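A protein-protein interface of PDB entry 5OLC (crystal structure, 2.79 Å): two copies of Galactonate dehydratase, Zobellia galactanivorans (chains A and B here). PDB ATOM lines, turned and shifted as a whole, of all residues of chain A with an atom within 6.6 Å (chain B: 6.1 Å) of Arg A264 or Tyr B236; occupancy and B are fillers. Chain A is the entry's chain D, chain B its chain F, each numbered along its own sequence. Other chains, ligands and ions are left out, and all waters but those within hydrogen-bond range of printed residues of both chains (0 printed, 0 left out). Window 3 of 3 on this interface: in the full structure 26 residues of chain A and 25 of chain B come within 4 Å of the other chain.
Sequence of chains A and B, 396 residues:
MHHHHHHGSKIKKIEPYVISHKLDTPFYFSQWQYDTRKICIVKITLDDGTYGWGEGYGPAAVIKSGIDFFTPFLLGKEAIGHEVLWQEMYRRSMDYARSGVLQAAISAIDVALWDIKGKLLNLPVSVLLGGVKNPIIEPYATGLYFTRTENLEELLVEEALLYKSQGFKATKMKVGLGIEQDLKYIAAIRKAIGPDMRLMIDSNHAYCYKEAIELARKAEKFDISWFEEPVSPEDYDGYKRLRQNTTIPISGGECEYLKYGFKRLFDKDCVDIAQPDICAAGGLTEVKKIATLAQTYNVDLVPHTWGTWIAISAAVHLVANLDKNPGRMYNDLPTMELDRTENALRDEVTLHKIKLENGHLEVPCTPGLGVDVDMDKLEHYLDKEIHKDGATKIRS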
ATOM      1  N   ARG A  98       5.097   3.364 -16.533  1.00  0.00           N
ATOM      2  CA  ARG A  98       5.545   4.599 -15.856  1.00  0.00           C
ATOM      3  C   ARG A  98       6.268   4.297 -14.536  1.00  0.00           C
ATOM      4  O   ARG A  98       7.330   4.867 -14.266  1.00  0.00           O
ATOM      5  CB  ARG A  98       4.401   5.611 -15.645  1.00  0.00           C
ATOM      6  CG  ARG A  98       3.757   6.119 -16.933  1.00  0.00           C
ATOM      7  CD  ARG A  98       2.822   7.271 -16.650  1.00  0.00           C
ATOM      8  NE  ARG A  98       3.553   8.462 -16.233  1.00  0.00           N
ATOM      9  CZ  ARG A  98       2.983   9.621 -15.935  1.00  0.00           C
ATOM     10  NH1 ARG A  98       3.730  10.664 -15.587  1.00  0.00           N
ATOM     11  NH2 ARG A  98       1.660   9.753 -15.995  1.00  0.00           N
ATOM     12  N   TYR A 236       6.296  14.437  -1.030  1.00  0.00           N
ATOM     13  CA  TYR A 236       7.467  15.234  -1.421  1.00  0.00           C
ATOM     14  C   TYR A 236       7.662  16.457  -0.511  1.00  0.00           C
ATOM     15  O   TYR A 236       8.792  16.741  -0.106  1.00  0.00           O
ATOM     16  CB  TYR A 236       7.383  15.683  -2.884  1.00  0.00           C
ATOM     17  CG  TYR A 236       7.315  14.566  -3.905  1.00  0.00           C
ATOM     18  CD1 TYR A 236       8.434  13.787  -4.197  1.00  0.00           C
ATOM     19  CD2 TYR A 236       6.168  14.365  -4.667  1.00  0.00           C
ATOM     20  CE1 TYR A 236       8.394  12.803  -5.188  1.00  0.00           C
ATOM     21  CE2 TYR A 236       6.119  13.391  -5.665  1.00  0.00           C
ATOM     22  CZ  TYR A 236       7.233  12.612  -5.923  1.00  0.00           C
ATOM     23  OH  TYR A 236       7.163  11.671  -6.928  1.00  0.00           O
ATOM     24  N   GLU A 256      11.019   5.253  -6.570  1.00  0.00           N
ATOM     25  CA  GLU A 256      11.048   6.148  -7.732  1.00  0.00           C
ATOM     26  C   GLU A 256      11.517   5.413  -8.977  1.00  0.00           C
ATOM     27  O   GLU A 256      12.469   4.636  -8.915  1.00  0.00           O
ATOM     28  CB  GLU A 256      11.858   7.420  -7.453  1.00  0.00           C
ATOM     29  CG  GLU A 256      11.096   8.494  -6.694  1.00  0.00           C
ATOM     30  CD  GLU A 256       9.960   9.174  -7.433  1.00  0.00           C
ATOM     31  OE1 GLU A 256       9.935   9.127  -8.683  1.00  0.00           O
ATOM     32  OE2 GLU A 256       9.094   9.765  -6.751  1.00  0.00           O
ATOM     33  N   LYS A 259      13.891   8.259 -15.376  1.00  0.00           N
ATOM     34  CA  LYS A 259      14.543   9.572 -15.380  1.00  0.00           C
ATOM     35  C   LYS A 259      13.507  10.656 -15.018  1.00  0.00           C
ATOM     36  O   LYS A 259      13.826  11.588 -14.271  1.00  0.00           O
ATOM     37  CB  LYS A 259      15.207   9.860 -16.761  1.00  0.00           C
ATOM     38  CG  LYS A 259      14.272   9.790 -18.000  1.00  0.00           C
ATOM     39  CD  LYS A 259      14.960  10.210 -19.302  1.00  0.00           C
ATOM     40  CE  LYS A 259      15.391   9.043 -20.156  1.00  0.00           C
ATOM     41  NZ  LYS A 259      14.224   8.320 -20.753  1.00  0.00           N
ATOM     42  N   TYR A 260      12.251  10.480 -15.499  1.00  0.00           N
ATOM     43  CA  TYR A 260      11.156  11.420 -15.286  1.00  0.00           C
ATOM     44  C   TYR A 260      10.736  11.487 -13.838  1.00  0.00           C
ATOM     45  O   TYR A 260      10.433  12.570 -13.332  1.00  0.00           O
ATOM     46  CB  TYR A 260       9.981  11.077 -16.182  1.00  0.00           C
ATOM     47  CG  TYR A 260      10.369  10.894 -17.630  1.00  0.00           C
ATOM     48  CD1 TYR A 260      10.498  11.986 -18.479  1.00  0.00           C
ATOM     49  CD2 TYR A 260      10.540   9.622 -18.172  1.00  0.00           C
ATOM     50  CE1 TYR A 260      10.802  11.821 -19.831  1.00  0.00           C
ATOM     51  CE2 TYR A 260      10.864   9.446 -19.519  1.00  0.00           C
ATOM     52  CZ  TYR A 260      11.003  10.551 -20.343  1.00  0.00           C
ATOM     53  OH  TYR A 260      11.325  10.399 -21.671  1.00  0.00           O
ATOM     54  N   GLY A 261      10.760  10.334 -13.183  1.00  0.00           N
ATOM     55  CA  GLY A 261      10.437  10.207 -11.774  1.00  0.00           C
ATOM     56  C   GLY A 261      11.491  10.855 -10.904  1.00  0.00           C
ATOM     57  O   GLY A 261      11.156  11.572  -9.961  1.00  0.00           O
ATOM     58  N   PHE A 262      12.773  10.648 -11.234  1.00  0.00           N
ATOM     59  CA  PHE A 262      13.847  11.242 -10.442  1.00  0.00           C
ATOM     60  C   PHE A 262      14.000  12.721 -10.690  1.00  0.00           C
ATOM     61  O   PHE A 262      14.365  13.439  -9.765  1.00  0.00           O
ATOM     62  CB  PHE A 262      15.167  10.491 -10.602  1.00  0.00           C
ATOM     63  CG  PHE A 262      15.294   9.418  -9.548  1.00  0.00           C
ATOM     64  CD1 PHE A 262      15.796   9.719  -8.286  1.00  0.00           C
ATOM     65  CD2 PHE A 262      14.844   8.128  -9.793  1.00  0.00           C
ATOM     66  CE1 PHE A 262      15.873   8.742  -7.299  1.00  0.00           C
ATOM     67  CE2 PHE A 262      14.928   7.150  -8.807  1.00  0.00           C
ATOM     68  CZ  PHE A 262      15.440   7.462  -7.564  1.00  0.00           C
ATOM     69  N   LYS A 263      13.630  13.196 -11.889  1.00  0.00           N
ATOM     70  CA  LYS A 263      13.652  14.624 -12.192  1.00  0.00           C
ATOM     71  C   LYS A 263      12.651  15.340 -11.255  1.00  0.00           C
ATOM     72  O   LYS A 263      13.023  16.343 -10.661  1.00  0.00           O
ATOM     73  CB  LYS A 263      13.364  14.848 -13.704  1.00  0.00           C
ATOM     74  CG  LYS A 263      12.524  16.050 -14.140  1.00  0.00           C
ATOM     75  CD  LYS A 263      13.285  17.347 -14.202  1.00  0.00           C
ATOM     76  CE  LYS A 263      12.645  18.320 -15.165  1.00  0.00           C
ATOM     77  NZ  LYS A 263      11.289  18.806 -14.772  1.00  0.00           N
ATOM     78  N   ARG A 264      11.416  14.781 -11.064  1.00  0.00           N
ATOM     79  CA  ARG A 264      10.408  15.382 -10.190  1.00  0.00           C
ATOM     80  C   ARG A 264      10.815  15.283  -8.738  1.00  0.00           C
ATOM     81  O   ARG A 264      10.497  16.197  -7.976  1.00  0.00           O
ATOM     82  CB  ARG A 264       8.969  14.890 -10.447  1.00  0.00           C
ATOM     83  CG  ARG A 264       8.580  13.496  -9.970  1.00  0.00           C
ATOM     84  CD  ARG A 264       7.133  13.172 -10.329  1.00  0.00           C
ATOM     85  NE  ARG A 264       6.938  12.429 -11.596  1.00  0.00           N
ATOM     86  CZ  ARG A 264       6.792  12.964 -12.819  1.00  0.00           C
ATOM     87  NH1 ARG A 264       6.579  12.183 -13.872  1.00  0.00           N
ATOM     88  NH2 ARG A 264       6.887  14.282 -12.996  1.00  0.00           N
ATOM     89  N   LEU A 265      11.576  14.241  -8.354  1.00  0.00           N
ATOM     90  CA  LEU A 265      12.064  14.144  -6.979  1.00  0.00           C
ATOM     91  C   LEU A 265      13.096  15.263  -6.697  1.00  0.00           C
ATOM     92  O   LEU A 265      13.015  15.944  -5.667  1.00  0.00           O
ATOM     93  CB  LEU A 265      12.666  12.756  -6.706  1.00  0.00           C
ATOM     94  CG  LEU A 265      13.238  12.516  -5.298  1.00  0.00           C
ATOM     95  CD1 LEU A 265      12.160  12.195  -4.316  1.00  0.00           C
ATOM     96  CD2 LEU A 265      14.223  11.402  -5.317  1.00  0.00           C
ATOM     97  N   PHE A 266      14.033  15.459  -7.631  1.00  0.00           N
ATOM     98  CA  PHE A 266      15.093  16.454  -7.527  1.00  0.00           C
ATOM     99  C   PHE A 266      14.594  17.889  -7.659  1.00  0.00           C
ATOM    100  O   PHE A 266      15.183  18.781  -7.032  1.00  0.00           O
ATOM    101  CB  PHE A 266      16.205  16.184  -8.565  1.00  0.00           C
ATOM    102  CG  PHE A 266      16.924  14.853  -8.506  1.00  0.00           C
ATOM    103  CD1 PHE A 266      17.329  14.312  -7.290  1.00  0.00           C
ATOM    104  CD2 PHE A 266      17.280  14.188  -9.671  1.00  0.00           C
ATOM    105  CE1 PHE A 266      18.008  13.097  -7.240  1.00  0.00           C
ATOM    106  CE2 PHE A 266      17.977  12.984  -9.619  1.00  0.00           C
ATOM    107  CZ  PHE A 266      18.337  12.445  -8.402  1.00  0.00           C
ATOM    108  N   ASP A 267      13.534  18.123  -8.475  1.00  0.00           N
ATOM    109  CA  ASP A 267      12.958  19.447  -8.701  1.00  0.00           C
ATOM    110  C   ASP A 267      12.362  20.007  -7.437  1.00  0.00           C
ATOM    111  O   ASP A 267      12.227  21.226  -7.320  1.00  0.00           O
ATOM    112  CB  ASP A 267      11.868  19.398  -9.778  1.00  0.00           C
ATOM    113  CG  ASP A 267      12.343  19.533 -11.210  1.00  0.00           C
ATOM    114  OD1 ASP A 267      13.528  19.812 -11.416  1.00  0.00           O
ATOM    115  OD2 ASP A 267      11.515  19.401 -12.116  1.00  0.00           O
ATOM    116  N   LYS A 268      11.997  19.122  -6.498  1.00  0.00           N
ATOM    117  CA  LYS A 268      11.368  19.491  -5.241  1.00  0.00           C
ATOM    118  C   LYS A 268      12.343  19.493  -4.057  1.00  0.00           C
ATOM    119  O   LYS A 268      11.891  19.580  -2.918  1.00  0.00           O
ATOM    120  CB  LYS A 268      10.128  18.607  -4.976  1.00  0.00           C
ATOM    121  CG  LYS A 268       9.068  18.642  -6.068  1.00  0.00           C
ATOM    122  CD  LYS A 268       7.692  18.412  -5.480  1.00  0.00           C
ATOM    123  CE  LYS A 268       6.619  18.627  -6.506  1.00  0.00           C
ATOM    124  NZ  LYS A 268       5.571  19.573  -6.015  1.00  0.00           N
ATOM    125  N   ASP A 269      13.671  19.426  -4.321  1.00  0.00           N
ATOM    126  CA  ASP A 269      14.747  19.449  -3.301  1.00  0.00           C
ATOM    127  C   ASP A 269      14.480  18.510  -2.068  1.00  0.00           C
ATOM    128  O   ASP A 269      14.766  18.873  -0.915  1.00  0.00           O
ATOM    129  CB  ASP A 269      15.025  20.909  -2.859  1.00  0.00           C
ATOM    130  CG  ASP A 269      16.491  21.281  -2.677  1.00  0.00           C
ATOM    131  OD1 ASP A 269      17.367  20.569  -3.245  1.00  0.00           O
ATOM    132  OD2 ASP A 269      16.769  22.288  -1.964  1.00  0.00           O
ATOM    133  N   CYS A 270      13.945  17.295  -2.344  1.00  0.00           N
ATOM    134  CA  CYS A 270      13.544  16.288  -1.359  1.00  0.00           C
ATOM    135  C   CYS A 270      14.691  15.613  -0.620  1.00  0.00           C
ATOM    136  O   CYS A 270      14.675  15.531   0.614  1.00  0.00           O
ATOM    137  CB  CYS A 270      12.647  15.242  -2.014  1.00  0.00           C
ATOM    138  SG  CYS A 270      11.262  15.928  -2.947  1.00  0.00           S
ATOM    139  N   TYR A 297      21.846  17.966 -10.923  1.00  0.00           N
ATOM    140  CA  TYR A 297      21.185  18.504  -9.733  1.00  0.00           C
ATOM    141  C   TYR A 297      22.102  18.526  -8.513  1.00  0.00           C
ATOM    142  O   TYR A 297      21.693  19.013  -7.461  1.00  0.00           O
ATOM    143  CB  TYR A 297      19.876  17.734  -9.423  1.00  0.00           C
ATOM    144  CG  TYR A 297      18.735  18.133 -10.328  1.00  0.00           C
ATOM    145  CD1 TYR A 297      18.607  17.588 -11.603  1.00  0.00           C
ATOM    146  CD2 TYR A 297      17.822  19.108  -9.943  1.00  0.00           C
ATOM    147  CE1 TYR A 297      17.596  17.999 -12.469  1.00  0.00           C
ATOM    148  CE2 TYR A 297      16.787  19.501 -10.791  1.00  0.00           C
ATOM    149  CZ  TYR A 297      16.683  18.944 -12.054  1.00  0.00           C
ATOM    150  OH  TYR A 297      15.690  19.313 -12.915  1.00  0.00           O
ATOM    151  N   VAL B 231       0.487  14.800 -26.477  1.00  0.00           N
ATOM    152  CA  VAL B 231       1.917  14.562 -26.283  1.00  0.00           C
ATOM    153  C   VAL B 231       2.116  13.465 -25.236  1.00  0.00           C
ATOM    154  O   VAL B 231       1.132  12.914 -24.733  1.00  0.00           O
ATOM    155  CB  VAL B 231       2.749  15.853 -25.969  1.00  0.00           C
ATOM    156  CG1 VAL B 231       2.645  16.873 -27.093  1.00  0.00           C
ATOM    157  CG2 VAL B 231       2.385  16.486 -24.633  1.00  0.00           C
ATOM    158  N   SER B 232       3.383  13.145 -24.912  1.00  0.00           N
ATOM    159  CA  SER B 232       3.745  12.152 -23.907  1.00  0.00           C
ATOM    160  C   SER B 232       3.080  12.463 -22.534  1.00  0.00           C
ATOM    161  O   SER B 232       3.148  13.612 -22.102  1.00  0.00           O
ATOM    162  CB  SER B 232       5.261  12.124 -23.751  1.00  0.00           C
ATOM    163  OG  SER B 232       5.677  11.327 -22.657  1.00  0.00           O
ATOM    164  N   PRO B 233       2.459  11.478 -21.825  1.00  0.00           N
ATOM    165  CA  PRO B 233       1.898  11.767 -20.481  1.00  0.00           C
ATOM    166  C   PRO B 233       2.939  12.284 -19.476  1.00  0.00           C
ATOM    167  O   PRO B 233       2.606  12.720 -18.379  1.00  0.00           O
ATOM    168  CB  PRO B 233       1.345  10.408 -20.029  1.00  0.00           C
ATOM    169  CG  PRO B 233       2.053   9.398 -20.863  1.00  0.00           C
ATOM    170  CD  PRO B 233       2.274  10.056 -22.187  1.00  0.00           C
ATOM    171  N   GLU B 234       4.201  12.237 -19.881  1.00  0.00           N
ATOM    172  CA  GLU B 234       5.387  12.660 -19.157  1.00  0.00           C
ATOM    173  C   GLU B 234       5.747  14.136 -19.446  1.00  0.00           C
ATOM    174  O   GLU B 234       6.412  14.777 -18.622  1.00  0.00           O
ATOM    175  CB  GLU B 234       6.537  11.741 -19.575  1.00  0.00           C
ATOM    176  CG  GLU B 234       7.261  11.119 -18.413  1.00  0.00           C
ATOM    177  CD  GLU B 234       6.597  10.089 -17.529  1.00  0.00           C
ATOM    178  OE1 GLU B 234       6.488   8.921 -17.963  1.00  0.00           O
ATOM    179  OE2 GLU B 234       6.375  10.403 -16.337  1.00  0.00           O
ATOM    180  N   ASP B 235       5.295  14.657 -20.617  1.00  0.00           N
ATOM    181  CA  ASP B 235       5.489  16.024 -21.102  1.00  0.00           C
ATOM    182  C   ASP B 235       4.412  16.978 -20.548  1.00  0.00           C
ATOM    183  O   ASP B 235       3.587  17.496 -21.312  1.00  0.00           O
ATOM    184  CB  ASP B 235       5.473  16.024 -22.645  1.00  0.00           C
ATOM    185  CG  ASP B 235       5.934  17.297 -23.348  1.00  0.00           C
ATOM    186  OD1 ASP B 235       6.538  18.183 -22.668  1.00  0.00           O
ATOM    187  OD2 ASP B 235       5.735  17.392 -24.582  1.00  0.00           O
ATOM    188  N   TYR B 236       4.426  17.221 -19.220  1.00  0.00           N
ATOM    189  CA  TYR B 236       3.460  18.109 -18.573  1.00  0.00           C
ATOM    190  C   TYR B 236       3.562  19.546 -19.093  1.00  0.00           C
ATOM    191  O   TYR B 236       2.538  20.160 -19.384  1.00  0.00           O
ATOM    192  CB  TYR B 236       3.635  18.095 -17.052  1.00  0.00           C
ATOM    193  CG  TYR B 236       3.419  16.752 -16.386  1.00  0.00           C
ATOM    194  CD1 TYR B 236       2.143  16.199 -16.282  1.00  0.00           C
ATOM    195  CD2 TYR B 236       4.469  16.087 -15.760  1.00  0.00           C
ATOM    196  CE1 TYR B 236       1.929  14.990 -15.618  1.00  0.00           C
ATOM    197  CE2 TYR B 236       4.265  14.884 -15.085  1.00  0.00           C
ATOM    198  CZ  TYR B 236       2.993  14.340 -15.013  1.00  0.00           C
ATOM    199  OH  TYR B 236       2.794  13.157 -14.341  1.00  0.00           O
ATOM    200  N   ASP B 237       4.802  20.066 -19.233  1.00  0.00           N
ATOM    201  CA  ASP B 237       5.065  21.411 -19.749  1.00  0.00           C
ATOM    202  C   ASP B 237       4.597  21.543 -21.195  1.00  0.00           C
ATOM    203  O   ASP B 237       4.189  22.628 -21.595  1.00  0.00           O
ATOM    204  CB  ASP B 237       6.546  21.804 -19.598  1.00  0.00           C
ATOM    205  CG  ASP B 237       7.042  22.064 -18.166  1.00  0.00           C
ATOM    206  OD1 ASP B 237       6.209  22.059 -17.229  1.00  0.00           O
ATOM    207  OD2 ASP B 237       8.265  22.275 -17.990  1.00  0.00           O
ATOM    208  N   GLY B 238       4.592  20.437 -21.935  1.00  0.00           N
ATOM    209  CA  GLY B 238       4.120  20.388 -23.312  1.00  0.00           C
ATOM    210  C   GLY B 238       2.621  20.551 -23.391  1.00  0.00           C
ATOM    211  O   GLY B 238       2.130  21.293 -24.241  1.00  0.00           O
ATOM    212  N   TYR B 239       1.894  19.864 -22.495  1.00  0.00           N
ATOM    213  CA  TYR B 239       0.447  19.920 -22.381  1.00  0.00           C
ATOM    214  C   TYR B 239       0.032  21.368 -22.096  1.00  0.00           C
ATOM    215  O   TYR B 239      -0.725  21.944 -22.881  1.00  0.00           O
ATOM    216  CB  TYR B 239      -0.031  19.001 -21.241  1.00  0.00           C
ATOM    217  CG  TYR B 239      -0.400  17.588 -21.657  1.00  0.00           C
ATOM    218  CD1 TYR B 239      -1.689  17.279 -22.081  1.00  0.00           C
ATOM    219  CD2 TYR B 239       0.506  16.541 -21.522  1.00  0.00           C
ATOM    220  CE1 TYR B 239      -2.042  15.983 -22.445  1.00  0.00           C
ATOM    221  CE2 TYR B 239       0.164  15.237 -21.879  1.00  0.00           C
ATOM    222  CZ  TYR B 239      -1.114  14.961 -22.344  1.00  0.00           C
ATOM    223  OH  TYR B 239      -1.469  13.676 -22.706  1.00  0.00           O
ATOM    224  N   LYS B 240       0.596  21.971 -21.013  1.00  0.00           N
ATOM    225  CA  LYS B 240       0.340  23.353 -20.576  1.00  0.00           C
ATOM    226  C   LYS B 240       0.536  24.363 -21.706  1.00  0.00           C
ATOM    227  O   LYS B 240      -0.336  25.216 -21.903  1.00  0.00           O
ATOM    228  CB  LYS B 240       1.193  23.738 -19.345  1.00  0.00           C
ATOM    229  CG  LYS B 240       0.693  25.013 -18.669  1.00  0.00           C
ATOM    230  CD  LYS B 240       1.488  25.407 -17.442  1.00  0.00           C
ATOM    231  CE  LYS B 240       0.809  26.557 -16.717  1.00  0.00           C
ATOM    232  NZ  LYS B 240       1.171  26.609 -15.272  1.00  0.00           N
ATOM    233  N   ARG B 241       1.678  24.265 -22.435  1.00  0.00           N
ATOM    234  CA  ARG B 241       2.022  25.142 -23.565  1.00  0.00           C
ATOM    235  C   ARG B 241       0.990  24.991 -24.704  1.00  0.00           C
ATOM    236  O   ARG B 241       0.526  25.992 -25.256  1.00  0.00           O
ATOM    237  CB  ARG B 241       3.426  24.816 -24.115  1.00  0.00           C
ATOM    238  CG  ARG B 241       4.631  25.479 -23.432  1.00  0.00           C
ATOM    239  CD  ARG B 241       5.917  25.346 -24.270  1.00  0.00           C
ATOM    240  NE  ARG B 241       6.154  23.980 -24.762  1.00  0.00           N
ATOM    241  CZ  ARG B 241       7.002  23.111 -24.219  1.00  0.00           C
ATOM    242  NH1 ARG B 241       7.728  23.451 -23.159  1.00  0.00           N
ATOM    243  NH2 ARG B 241       7.139  21.896 -24.738  1.00  0.00           N
ATOM    244  N   GLU B 256      -2.523   8.367 -16.248  1.00  0.00           N
ATOM    245  CA  GLU B 256      -2.420   8.918 -14.904  1.00  0.00           C
ATOM    246  C   GLU B 256      -3.086   8.003 -13.901  1.00  0.00           C
ATOM    247  O   GLU B 256      -4.196   7.524 -14.150  1.00  0.00           O
ATOM    248  CB  GLU B 256      -2.938  10.356 -14.851  1.00  0.00           C
ATOM    249  CG  GLU B 256      -1.942  11.382 -15.361  1.00  0.00           C
ATOM    250  CD  GLU B 256      -0.708  11.563 -14.495  1.00  0.00           C
ATOM    251  OE1 GLU B 256      -0.788  11.309 -13.269  1.00  0.00           O
ATOM    252  OE2 GLU B 256       0.338  11.973 -15.049  1.00  0.00           O
ATOM    253  N   GLY B 261      -1.231  11.106  -8.539  1.00  0.00           N
ATOM    254  CA  GLY B 261      -0.843  11.348  -9.921  1.00  0.00           C
ATOM    255  C   GLY B 261      -1.642  12.467 -10.536  1.00  0.00           C
ATOM    256  O   GLY B 261      -1.067  13.405 -11.078  1.00  0.00           O
ATOM    257  N   ARG B 264      -0.744  15.915  -9.135  1.00  0.00           N
ATOM    258  CA  ARG B 264       0.504  16.326  -9.779  1.00  0.00           C
ATOM    259  C   ARG B 264       0.223  16.930 -11.164  1.00  0.00           C
ATOM    260  O   ARG B 264       0.841  17.942 -11.521  1.00  0.00           O
ATOM    261  CB  ARG B 264       1.539  15.157  -9.778  1.00  0.00           C
ATOM    262  CG  ARG B 264       2.483  15.008 -11.012  1.00  0.00           C
ATOM    263  CD  ARG B 264       3.563  13.905 -10.918  1.00  0.00           C
ATOM    264  NE  ARG B 264       3.117  12.618 -10.339  1.00  0.00           N
ATOM    265  CZ  ARG B 264       3.535  12.127  -9.166  1.00  0.00           C
ATOM    266  NH1 ARG B 264       3.083  10.959  -8.728  1.00  0.00           N
ATOM    267  NH2 ARG B 264       4.410  12.799  -8.430  1.00  0.00           N
ATOM    268  N   LEU B 265      -0.726  16.329 -11.909  1.00  0.00           N
ATOM    269  CA  LEU B 265      -1.139  16.759 -13.235  1.00  0.00           C
ATOM    270  C   LEU B 265      -1.902  18.096 -13.186  1.00  0.00           C
ATOM    271  O   LEU B 265      -1.575  19.008 -13.961  1.00  0.00           O
ATOM    272  CB  LEU B 265      -1.967  15.635 -13.868  1.00  0.00           C
ATOM    273  CG  LEU B 265      -2.809  15.960 -15.084  1.00  0.00           C
ATOM    274  CD1 LEU B 265      -2.031  15.754 -16.342  1.00  0.00           C
ATOM    275  CD2 LEU B 265      -4.014  15.064 -15.130  1.00  0.00           C
ATOM    276  N   LYS B 268      -0.232  21.405 -12.493  1.00  0.00           N
ATOM    277  CA  LYS B 268       0.533  21.870 -13.627  1.00  0.00           C
ATOM    278  C   LYS B 268      -0.338  22.513 -14.698  1.00  0.00           C
ATOM    279  O   LYS B 268       0.174  22.936 -15.727  1.00  0.00           O
ATOM    280  CB  LYS B 268       1.393  20.710 -14.160  1.00  0.00           C
ATOM    281  CG  LYS B 268       2.410  20.142 -13.137  1.00  0.00           C
ATOM    282  CD  LYS B 268       3.636  21.062 -12.853  1.00  0.00           C
ATOM    283  CE  LYS B 268       4.713  21.005 -13.923  1.00  0.00           C
ATOM    284  NZ  LYS B 268       6.040  21.402 -13.387  1.00  0.00           N
ATOM    285  N   CYS B 270      -2.353  21.275 -16.857  1.00  0.00           N
ATOM    286  CA  CYS B 270      -2.177  20.514 -18.109  1.00  0.00           C
ATOM    287  C   CYS B 270      -3.430  20.368 -18.977  1.00  0.00           C
ATOM    288  O   CYS B 270      -3.392  20.633 -20.189  1.00  0.00           O
ATOM    289  CB  CYS B 270      -1.580  19.140 -17.816  1.00  0.00           C
ATOM    290  SG  CYS B 270      -0.085  19.168 -16.800  1.00  0.00           S
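OE2 of Glu B234 is in salt-bridge range of NH1 of Arg A98 (2.8 Å). The guanidinium group (NH1) of Arg A98 lies within hydrogen-bond range of the side-chain hydroxyl (OH) of Tyr B236 (2.9 Å). The side-chain carboxylate (OE2) of Glu B256 lies within salt-bridge range of the guanidinium group (NH2) of Arg A98, 2.8 Å away. NH2 of Arg B264 lies close to OH of Tyr A236 (3.3 Å). NH1 of Arg A264 is in salt-bridge range of OE2 of Glu B234 (3.0 Å).
The side-chain hydroxyl of Tyr A236 is in hydrogen-bond range of the side-chain carboxylate of Glu A256, 2.7 Å away. The backbone NH of Glu B234 lies close to the side-chain hydroxyl of Ser B232 (3.3 Å). The side-chain hydroxyl of Tyr B236 lies within hydrogen-bond range of the side-chain carboxylate of Glu B256, 2.8 Å away.
Among the printed residues, merely in contact across the chains: Arg A98 with Pro B233 (3.6 Å), Tyr A260 with Glu B234 (3.2 Å), Arg A264 with Tyr B236 (3.4 Å) and Arg A264 with Arg B264 (3.3 Å).
Printed residues of chain B within 4 Å of Tyr A236: Arg B264. Of the printed residues of chain B, Arg A264 touches Glu B234 (3.0 Å), Tyr B236 (3.4 Å) and Arg B264 (3.3 Å). Of the printed residues of chain A, Pro B233 touches Arg A98. Of the printed residues of chain A, Glu B234 touches Arg A98 (2.8 Å), Tyr A260 (3.2 Å) and Arg A264 (3.0 Å). Tyr B236 touches just these residues of chain A: Arg A98 (2.9 Å) and Arg A264 (3.4 Å). Printed residues of chain A within 4 Å of Arg B264: Tyr A236 and Arg A264. The nearest printed residue of chain A that does not touch Tyr B236 is Tyr A260 (6.8 Å).
Of the 17 printed residues of chain B, 5 touch a printed residue of chain A. Hydrophobic or aromatic side chains of chain B that line the printed part of chain A: Tyr B236. Along chain B the printed residues that touch a printed residue of chain A span positions 233 to 264. Of the 16 printed residues of chain A, 4 touch a printed residue of chain B. Hydrophobic or aromatic side chains of chain A that line the printed part of chain B: Tyr A236 and Tyr A260. Along chain A the printed residues that touch a printed residue of chain B span positions 98 to 264. Among the printed residues, 9 pairs touch across the chains. Among the printed residues, Asp or Glu carboxylates within 4 Å of a Lys or Arg side-chain nitrogen of the other chain: Arg A98 with Glu B234, Arg A98 with Glu B256 and Arg A264 with Glu B234.
Tyr A236 touches Arg B264, and with the chains exchanged Arg A264 touches Tyr B236. Arg B264 touches its own counterpart, Arg A264. Positions printed for both chains: 236, 256, 261, 264, 265, 268 and 270. Of the 9 pairs that touch across the chains among the printed residues, 3 have their exchanged pair printed and touching as well.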
